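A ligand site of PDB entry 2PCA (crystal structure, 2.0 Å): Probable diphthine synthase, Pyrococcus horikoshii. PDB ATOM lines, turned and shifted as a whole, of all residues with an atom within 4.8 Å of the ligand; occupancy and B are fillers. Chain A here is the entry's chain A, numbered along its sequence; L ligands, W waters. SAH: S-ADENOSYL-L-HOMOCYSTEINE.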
ATOM      1  N   LEU A  10      -0.524 -24.478 -15.594  1.00  0.00           N
ATOM      2  CA  LEU A  10       0.148 -23.306 -15.040  1.00  0.00           C
ATOM      3  C   LEU A  10       1.679 -23.424 -15.006  1.00  0.00           C
ATOM      4  O   LEU A  10       2.402 -22.507 -15.385  1.00  0.00           O
ATOM      5  CB  LEU A  10      -0.373 -23.093 -13.629  1.00  0.00           C
ATOM      6  CG  LEU A  10      -1.792 -22.503 -13.595  1.00  0.00           C
ATOM      7  CD1 LEU A  10      -2.411 -22.548 -12.198  1.00  0.00           C
ATOM      8  CD2 LEU A  10      -1.838 -21.047 -14.045  1.00  0.00           C
ATOM      9  N   THR A  36       3.457 -17.463 -25.356  1.00  0.00           N
ATOM     10  CA  THR A  36       2.390 -16.725 -24.693  1.00  0.00           C
ATOM     11  C   THR A  36       2.517 -16.736 -23.173  1.00  0.00           C
ATOM     12  O   THR A  36       1.880 -15.955 -22.483  1.00  0.00           O
ATOM     13  CB  THR A  36       0.988 -17.279 -25.069  1.00  0.00           C
ATOM     14  OG1 THR A  36       0.907 -18.677 -24.734  1.00  0.00           O
ATOM     15  CG2 THR A  36       0.734 -17.094 -26.560  1.00  0.00           C
ATOM     16  N   SER A  37       3.361 -17.626 -22.644  1.00  0.00           N
ATOM     17  CA  SER A  37       3.562 -17.709 -21.216  1.00  0.00           C
ATOM     18  C   SER A  37       4.771 -18.567 -20.895  1.00  0.00           C
ATOM     19  O   SER A  37       5.350 -19.182 -21.789  1.00  0.00           O
ATOM     20  CB  SER A  37       2.315 -18.307 -20.545  1.00  0.00           C
ATOM     21  OG  SER A  37       2.399 -18.187 -19.128  1.00  0.00           O
ATOM     22  N   LEU A  38       5.145 -18.614 -19.626  1.00  0.00           N
ATOM     23  CA  LEU A  38       6.289 -19.404 -19.193  1.00  0.00           C
ATOM     24  C   LEU A  38       5.894 -20.503 -18.207  1.00  0.00           C
ATOM     25  O   LEU A  38       5.302 -20.224 -17.165  1.00  0.00           O
ATOM     26  CB  LEU A  38       7.345 -18.516 -18.542  1.00  0.00           C
ATOM     27  CG  LEU A  38       8.535 -19.232 -17.905  1.00  0.00           C
ATOM     28  CD1 LEU A  38       9.343 -19.933 -18.989  1.00  0.00           C
ATOM     29  CD2 LEU A  38       9.411 -18.242 -17.156  1.00  0.00           C
ATOM     30  N   PRO A  85       0.565 -22.999 -23.009  1.00  0.00           N
ATOM     31  CA  PRO A  85       0.666 -22.889 -21.552  1.00  0.00           C
ATOM     32  C   PRO A  85      -0.703 -22.440 -21.028  1.00  0.00           C
ATOM     33  O   PRO A  85      -1.466 -21.794 -21.760  1.00  0.00           O
ATOM     34  CB  PRO A  85       1.725 -21.804 -21.356  1.00  0.00           C
ATOM     35  CG  PRO A  85       2.582 -21.944 -22.589  1.00  0.00           C
ATOM     36  CD  PRO A  85       1.559 -22.135 -23.675  1.00  0.00           C
ATOM     37  N   GLY A  86      -1.006 -22.781 -19.778  1.00  0.00           N
ATOM     38  CA  GLY A  86      -2.284 -22.398 -19.181  1.00  0.00           C
ATOM     39  C   GLY A  86      -3.472 -22.847 -20.024  1.00  0.00           C
ATOM     40  O   GLY A  86      -3.482 -23.969 -20.517  1.00  0.00           O
ATOM     41  N   ASP A  87      -4.479 -21.980 -20.153  1.00  0.00           N
ATOM     42  CA  ASP A  87      -5.649 -22.271 -20.975  1.00  0.00           C
ATOM     43  C   ASP A  87      -5.336 -21.619 -22.313  1.00  0.00           C
ATOM     44  O   ASP A  87      -4.934 -20.458 -22.359  1.00  0.00           O
ATOM     45  CB  ASP A  87      -6.907 -21.655 -20.353  1.00  0.00           C
ATOM     46  CG  ASP A  87      -8.159 -21.950 -21.160  1.00  0.00           C
ATOM     47  OD1 ASP A  87      -8.274 -21.438 -22.299  1.00  0.00           O
ATOM     48  OD2 ASP A  87      -9.028 -22.674 -20.642  1.00  0.00           O
ATOM     49  N   VAL A  90      -7.046 -17.959 -23.089  1.00  0.00           N
ATOM     50  CA  VAL A  90      -6.970 -16.897 -22.087  1.00  0.00           C
ATOM     51  C   VAL A  90      -5.788 -15.946 -22.252  1.00  0.00           C
ATOM     52  O   VAL A  90      -4.630 -16.344 -22.100  1.00  0.00           O
ATOM     53  CB  VAL A  90      -6.902 -17.494 -20.667  1.00  0.00           C
ATOM     54  CG1 VAL A  90      -6.679 -16.380 -19.648  1.00  0.00           C
ATOM     55  CG2 VAL A  90      -8.178 -18.266 -20.354  1.00  0.00           C
ATOM     56  N   ALA A  91      -6.094 -14.695 -22.551  1.00  0.00           N
ATOM     57  CA  ALA A  91      -5.055 -13.676 -22.719  1.00  0.00           C
ATOM     58  C   ALA A  91      -4.105 -14.018 -23.858  1.00  0.00           C
ATOM     59  O   ALA A  91      -2.897 -13.829 -23.743  1.00  0.00           O
ATOM     60  CB  ALA A  91      -4.281 -13.499 -21.424  1.00  0.00           C
ATOM     61  N   THR A  92      -4.678 -14.554 -24.927  1.00  0.00           N
ATOM     62  CA  THR A  92      -3.936 -14.891 -26.142  1.00  0.00           C
ATOM     63  C   THR A  92      -4.918 -14.482 -27.222  1.00  0.00           C
ATOM     64  O   THR A  92      -6.037 -14.074 -26.916  1.00  0.00           O
ATOM     65  CB  THR A  92      -3.689 -16.392 -26.303  1.00  0.00           C
ATOM     66  OG1 THR A  92      -4.949 -17.052 -26.473  1.00  0.00           O
ATOM     67  CG2 THR A  92      -2.961 -16.975 -25.091  1.00  0.00           C
ATOM     68  N   PRO A 114      -5.787 -25.442 -16.065  1.00  0.00           N
ATOM     69  CA  PRO A 114      -5.756 -24.328 -15.115  1.00  0.00           C
ATOM     70  C   PRO A 114      -5.095 -23.087 -15.702  1.00  0.00           C
ATOM     71  O   PRO A 114      -4.074 -23.184 -16.384  1.00  0.00           O
ATOM     72  CB  PRO A 114      -4.990 -24.910 -13.916  1.00  0.00           C
ATOM     73  CG  PRO A 114      -5.053 -26.413 -14.022  1.00  0.00           C
ATOM     74  CD  PRO A 114      -5.134 -26.638 -15.512  1.00  0.00           C
ATOM     75  N   SER A 115      -5.690 -21.934 -15.436  1.00  0.00           N
ATOM     76  CA  SER A 115      -5.210 -20.648 -15.944  1.00  0.00           C
ATOM     77  C   SER A 115      -4.874 -19.685 -14.828  1.00  0.00           C
ATOM     78  O   SER A 115      -5.461 -19.730 -13.754  1.00  0.00           O
ATOM     79  CB  SER A 115      -6.291 -20.024 -16.830  1.00  0.00           C
ATOM     80  OG  SER A 115      -5.980 -18.670 -17.119  1.00  0.00           O
ATOM     81  N   ILE A 116      -3.925 -18.795 -15.099  1.00  0.00           N
ATOM     82  CA  ILE A 116      -3.534 -17.798 -14.105  1.00  0.00           C
ATOM     83  C   ILE A 116      -4.746 -16.937 -13.759  1.00  0.00           C
ATOM     84  O   ILE A 116      -4.863 -16.435 -12.639  1.00  0.00           O
ATOM     85  CB  ILE A 116      -2.373 -16.901 -14.626  1.00  0.00           C
ATOM     86  CG1 ILE A 116      -1.833 -16.017 -13.501  1.00  0.00           C
ATOM     87  CG2 ILE A 116      -2.843 -16.022 -15.784  1.00  0.00           C
ATOM     88  CD1 ILE A 116      -1.198 -16.789 -12.356  1.00  0.00           C
ATOM     89  N   TYR A 117      -5.664 -16.778 -14.714  1.00  0.00           N
ATOM     90  CA  TYR A 117      -6.841 -15.952 -14.479  1.00  0.00           C
ATOM     91  C   TYR A 117      -7.678 -16.437 -13.286  1.00  0.00           C
ATOM     92  O   TYR A 117      -8.204 -15.630 -12.519  1.00  0.00           O
ATOM     93  CB  TYR A 117      -7.707 -15.879 -15.740  1.00  0.00           C
ATOM     94  CG  TYR A 117      -8.740 -14.776 -15.702  1.00  0.00           C
ATOM     95  CD1 TYR A 117      -8.365 -13.427 -15.709  1.00  0.00           C
ATOM     96  CD2 TYR A 117     -10.104 -15.075 -15.613  1.00  0.00           C
ATOM     97  CE1 TYR A 117      -9.312 -12.417 -15.632  1.00  0.00           C
ATOM     98  CE2 TYR A 117     -11.063 -14.070 -15.542  1.00  0.00           C
ATOM     99  CZ  TYR A 117     -10.661 -12.733 -15.545  1.00  0.00           C
ATOM    100  OH  TYR A 117     -11.614 -11.747 -15.471  1.00  0.00           O
ATOM    101  N   PHE A 165      -1.311  -8.799 -15.980  1.00  0.00           N
ATOM    102  CA  PHE A 165      -0.487  -9.791 -16.657  1.00  0.00           C
ATOM    103  C   PHE A 165       0.832  -9.058 -16.888  1.00  0.00           C
ATOM    104  O   PHE A 165       0.832  -7.848 -17.143  1.00  0.00           O
ATOM    105  CB  PHE A 165      -1.106 -10.177 -17.994  1.00  0.00           C
ATOM    106  CG  PHE A 165      -2.427 -10.905 -17.882  1.00  0.00           C
ATOM    107  CD1 PHE A 165      -2.467 -12.241 -17.509  1.00  0.00           C
ATOM    108  CD2 PHE A 165      -3.627 -10.251 -18.157  1.00  0.00           C
ATOM    109  CE1 PHE A 165      -3.686 -12.927 -17.417  1.00  0.00           C
ATOM    110  CE2 PHE A 165      -4.850 -10.927 -18.066  1.00  0.00           C
ATOM    111  CZ  PHE A 165      -4.868 -12.268 -17.699  1.00  0.00           C
ATOM    112  N   LEU A 166       1.948  -9.757 -16.812  1.00  0.00           N
ATOM    113  CA  LEU A 166       3.238  -9.107 -17.036  1.00  0.00           C
ATOM    114  C   LEU A 166       3.783  -9.498 -18.402  1.00  0.00           C
ATOM    115  O   LEU A 166       3.523 -10.598 -18.897  1.00  0.00           O
ATOM    116  CB  LEU A 166       4.209  -9.449 -15.904  1.00  0.00           C
ATOM    117  CG  LEU A 166       3.694  -9.075 -14.501  1.00  0.00           C
ATOM    118  CD1 LEU A 166       4.821  -9.176 -13.475  1.00  0.00           C
ATOM    119  CD2 LEU A 166       3.150  -7.642 -14.500  1.00  0.00           C
ATOM    120  N   ASP A 167       4.523  -8.588 -19.032  1.00  0.00           N
ATOM    121  CA  ASP A 167       5.048  -8.821 -20.364  1.00  0.00           C
ATOM    122  C   ASP A 167       6.007  -9.995 -20.503  1.00  0.00           C
ATOM    123  O   ASP A 167       6.670 -10.409 -19.537  1.00  0.00           O
ATOM    124  CB  ASP A 167       5.720  -7.549 -20.898  1.00  0.00           C
ATOM    125  CG  ASP A 167       5.618  -7.422 -22.411  1.00  0.00           C
ATOM    126  OD1 ASP A 167       5.081  -8.337 -23.057  1.00  0.00           O
ATOM    127  OD2 ASP A 167       6.072  -6.393 -22.947  1.00  0.00           O
ATOM    128  N   ILE A 168       6.080 -10.534 -21.708  1.00  0.00           N
ATOM    129  CA  ILE A 168       6.958 -11.659 -21.994  1.00  0.00           C
ATOM    130  C   ILE A 168       7.519 -11.550 -23.409  1.00  0.00           C
ATOM    131  O   ILE A 168       6.789 -11.251 -24.348  1.00  0.00           O
ATOM    132  CB  ILE A 168       6.193 -13.010 -21.821  1.00  0.00           C
ATOM    133  CG1 ILE A 168       7.044 -14.165 -22.349  1.00  0.00           C
ATOM    134  CG2 ILE A 168       4.852 -12.939 -22.526  1.00  0.00           C
ATOM    135  CD1 ILE A 168       6.390 -15.530 -22.154  1.00  0.00           C
ATOM    136  N   LEU A 206       2.036 -12.818  -7.144  1.00  0.00           N
ATOM    137  CA  LEU A 206       1.863 -14.260  -7.230  1.00  0.00           C
ATOM    138  C   LEU A 206       2.886 -14.730  -8.243  1.00  0.00           C
ATOM    139  O   LEU A 206       2.846 -14.324  -9.412  1.00  0.00           O
ATOM    140  CB  LEU A 206       0.443 -14.629  -7.688  1.00  0.00           C
ATOM    141  CG  LEU A 206       0.136 -16.122  -7.903  1.00  0.00           C
ATOM    142  CD1 LEU A 206       0.505 -16.918  -6.659  1.00  0.00           C
ATOM    143  CD2 LEU A 206      -1.332 -16.310  -8.238  1.00  0.00           C
ATOM    144  N   ALA A 207       3.823 -15.557  -7.802  1.00  0.00           N
ATOM    145  CA  ALA A 207       4.876 -16.063  -8.676  1.00  0.00           C
ATOM    146  C   ALA A 207       4.858 -17.580  -8.761  1.00  0.00           C
ATOM    147  O   ALA A 207       4.789 -18.265  -7.739  1.00  0.00           O
ATOM    148  CB  ALA A 207       6.239 -15.582  -8.195  1.00  0.00           C
ATOM    149  N   ARG A 208       4.912 -18.086  -9.990  1.00  0.00           N
ATOM    150  CA  ARG A 208       4.918 -19.521 -10.242  1.00  0.00           C
ATOM    151  C   ARG A 208       3.690 -20.247  -9.707  1.00  0.00           C
ATOM    152  O   ARG A 208       3.797 -21.294  -9.051  1.00  0.00           O
ATOM    153  CB  ARG A 208       6.203 -20.138  -9.658  1.00  0.00           C
ATOM    154  CG  ARG A 208       7.489 -19.452 -10.157  1.00  0.00           C
ATOM    155  CD  ARG A 208       8.731 -20.075  -9.516  1.00  0.00           C
ATOM    156  NE  ARG A 208       8.611 -20.082  -8.059  1.00  0.00           N
ATOM    157  CZ  ARG A 208       8.704 -19.003  -7.292  1.00  0.00           C
ATOM    158  NH1 ARG A 208       8.932 -17.806  -7.830  1.00  0.00           N
ATOM    159  NH2 ARG A 208       8.535 -19.109  -5.979  1.00  0.00           N
ATOM    160  N   ALA A 209       2.509 -19.691  -9.976  1.00  0.00           N
ATOM    161  CA  ALA A 209       1.266 -20.321  -9.557  1.00  0.00           C
ATOM    162  C   ALA A 209       1.307 -21.693 -10.221  1.00  0.00           C
ATOM    163  O   ALA A 209       1.867 -21.839 -11.306  1.00  0.00           O
ATOM    164  CB  ALA A 209       0.065 -19.518 -10.071  1.00  0.00           C
ATOM    165  N   PRO A 233       7.260 -17.193 -14.039  1.00  0.00           N
ATOM    166  CA  PRO A 233       6.448 -15.995 -14.252  1.00  0.00           C
ATOM    167  C   PRO A 233       5.827 -15.379 -13.002  1.00  0.00           C
ATOM    168  O   PRO A 233       5.629 -16.057 -11.995  1.00  0.00           O
ATOM    169  CB  PRO A 233       5.378 -16.495 -15.229  1.00  0.00           C
ATOM    170  CG  PRO A 233       5.121 -17.874 -14.703  1.00  0.00           C
ATOM    171  CD  PRO A 233       6.515 -18.408 -14.409  1.00  0.00           C
ATOM    172  N   HIS A 234       5.531 -14.088 -13.098  1.00  0.00           N
ATOM    173  CA  HIS A 234       4.924 -13.339 -12.002  1.00  0.00           C
ATOM    174  C   HIS A 234       3.712 -12.583 -12.524  1.00  0.00           C
ATOM    175  O   HIS A 234       3.626 -12.281 -13.718  1.00  0.00           O
ATOM    176  CB  HIS A 234       5.872 -12.256 -11.460  1.00  0.00           C
ATOM    177  CG  HIS A 234       7.152 -12.760 -10.891  1.00  0.00           C
ATOM    178  ND1 HIS A 234       8.120 -11.909 -10.385  1.00  0.00           N
ATOM    179  CD2 HIS A 234       7.625 -14.012 -10.708  1.00  0.00           C
ATOM    180  CE1 HIS A 234       9.129 -12.614  -9.920  1.00  0.00           C
ATOM    181  NE2 HIS A 234       8.854 -13.900 -10.098  1.00  0.00           N
ATOM    182  N   ILE A 235       2.780 -12.278 -11.628  1.00  0.00           N
ATOM    183  CA  ILE A 235       1.652 -11.428 -11.973  1.00  0.00           C
ATOM    184  C   ILE A 235       1.599 -10.453 -10.824  1.00  0.00           C
ATOM    185  O   ILE A 235       2.027 -10.778  -9.709  1.00  0.00           O
ATOM    186  CB  ILE A 235       0.275 -12.148 -12.060  1.00  0.00           C
ATOM    187  CG1 ILE A 235      -0.040 -12.844 -10.732  1.00  0.00           C
ATOM    188  CG2 ILE A 235       0.249 -13.079 -13.237  1.00  0.00           C
ATOM    189  CD1 ILE A 235      -1.535 -13.147 -10.581  1.00  0.00           C
HETATM  190  N   SAH L   1      -3.190 -18.498 -21.393  1.00  0.00           N
HETATM  191  CA  SAH L   1      -2.346 -18.170 -20.177  1.00  0.00           C
HETATM  192  CB  SAH L   1      -1.947 -16.731 -19.966  1.00  0.00           C
HETATM  193  CG  SAH L   1      -1.155 -16.003 -21.063  1.00  0.00           C
HETATM  194  SD  SAH L   1      -0.567 -14.395 -20.372  1.00  0.00           S
HETATM  195  C   SAH L   1      -3.139 -18.729 -18.926  1.00  0.00           C
HETATM  196  O   SAH L   1      -4.250 -19.277 -19.115  1.00  0.00           O
HETATM  197  OXT SAH L   1      -2.590 -18.571 -17.771  1.00  0.00           O
HETATM  198  C5' SAH L   1       1.007 -14.857 -19.754  1.00  0.00           C
HETATM  199  C4' SAH L   1       1.314 -14.018 -18.459  1.00  0.00           C
HETATM  200  O4' SAH L   1       0.400 -14.456 -17.436  1.00  0.00           O
HETATM  201  C3' SAH L   1       2.690 -14.159 -17.888  1.00  0.00           C
HETATM  202  O3' SAH L   1       3.584 -13.246 -18.491  1.00  0.00           O
HETATM  203  C2' SAH L   1       2.427 -13.922 -16.391  1.00  0.00           C
HETATM  204  O2' SAH L   1       2.397 -12.526 -16.058  1.00  0.00           O
HETATM  205  C1' SAH L   1       1.096 -14.656 -16.134  1.00  0.00           C
HETATM  206  N9  SAH L   1       1.209 -15.971 -15.836  1.00  0.00           N
HETATM  207  C8  SAH L   1       0.979 -17.141 -16.539  1.00  0.00           C
HETATM  208  N7  SAH L   1       1.213 -18.229 -15.870  1.00  0.00           N
HETATM  209  C5  SAH L   1       1.638 -17.789 -14.593  1.00  0.00           C
HETATM  210  C6  SAH L   1       2.028 -18.512 -13.414  1.00  0.00           C
HETATM  211  N6  SAH L   1       2.068 -19.848 -13.324  1.00  0.00           N
HETATM  212  N1  SAH L   1       2.376 -17.720 -12.336  1.00  0.00           N
HETATM  213  C2  SAH L   1       2.359 -16.359 -12.375  1.00  0.00           C
HETATM  214  N3  SAH L   1       1.984 -15.632 -13.483  1.00  0.00           N
HETATM  215  C4  SAH L   1       1.635 -16.413 -14.553  1.00  0.00           C
HETATM  216  O   HOH W   1      -0.261 -20.166 -17.828  1.00  0.00           O
HETATM  217  O   HOH W   2       6.438 -13.076 -18.283  1.00  0.00           O
HETATM  218  O   HOH W   3      -0.812 -19.275 -22.949  1.00  0.00           O
HETATM  219  O   HOH W   4       2.632 -20.491 -17.687  1.00  0.00           O
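N of the ligand sits at hydrogen-bond distance from O of Asp 87, at 2.8 Å.
The side-chain hydroxyl of Ser 37 lies close to a nitrogen (N7) of the ligand, 3.5 Å away.
O of the ligand lies within hydrogen-bond range of N of Asp 87 (2.9 Å).
A nitrogen (N1) of the ligand sits at hydrogen-bond distance from the backbone NH (N) of Ala 209 (3.1 Å).
The backbone carbonyl oxygen (O) of Leu 166 sits at hydrogen-bond distance from an oxygen (O3') of the ligand, 2.7 Å away.
The side-chain hydroxyl of Ser 115 lies within hydrogen-bond range of an oxygen (O) of the ligand (2.7 Å).
N of the ligand is in hydrogen-bond range of O of Val 90, 2.7 Å away.
The backbone carbonyl oxygen (O) of Leu 10 sits at hydrogen-bond distance from a nitrogen (N6) of the ligand, at 3.4 Å.
O of His 234 is in hydrogen-bond range of O2' of the ligand, 2.7 Å away.
N1 of the ligand is in hydrogen-bond range of N of Arg 208 (3.5 Å).
N of Ile 116 lies within hydrogen-bond range of OXT of the ligand (3.0 Å).
The backbone carbonyl oxygen (O) of Ala 209 sits at hydrogen-bond distance from a nitrogen (N6) of the ligand (2.8 Å).
The backbone NH (N) of Leu 166 sits at hydrogen-bond distance from an oxygen (O2') of the ligand, at 2.9 Å.
N of Ile 235 lies within hydrogen-bond range of O of Leu 206, 3.0 Å away.
O of Pro 233 lies within hydrogen-bond range of N of Arg 208 (2.9 Å).
The side-chain hydroxyl of Ser 115 sits close to the backbone NH of Tyr 117 (3.1 Å).
The backbone carbonyl oxygen (O) of Thr 36 sits close to a sulfur (SD) of the ligand, 3.6 Å away.
Merely in contact with the ligand: Pro 85, Gly 86, Ala 91, Phe 165, Leu 206, Pro 233 and Ile 235.
Hydrophobic or aromatic side chains within 4 Å of the ligand: Val 90, Ala 91, Ile 116, Phe 165, Leu 166, Ala 209, Pro 233 and Ile 235.
Within 4 Å of the ligand: Leu 10, Thr 36, Ser 37, Pro 85, Gly 86, Asp 87, Val 90, Ala 91, Ser 115, Ile 116, Phe 165, Leu 166, Leu 206, Arg 208, Ala 209, Pro 233, His 234 and Ile 235.
Water W1 lies within hydrogen-bond range of OXT of the ligand (2.8 Å) and N of Gly 86 (3.3 Å).
Water W2 bridges O3' of the ligand (2.9 Å) and O of Asp 167 (3.0 Å).
Water W3 lies within hydrogen-bond range of the side-chain hydroxyl (OG1) of Thr 36 (2.5 Å), the backbone carbonyl oxygen (O) of Pro 85 (2.9 Å) and a nitrogen (N) of the ligand (2.9 Å).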
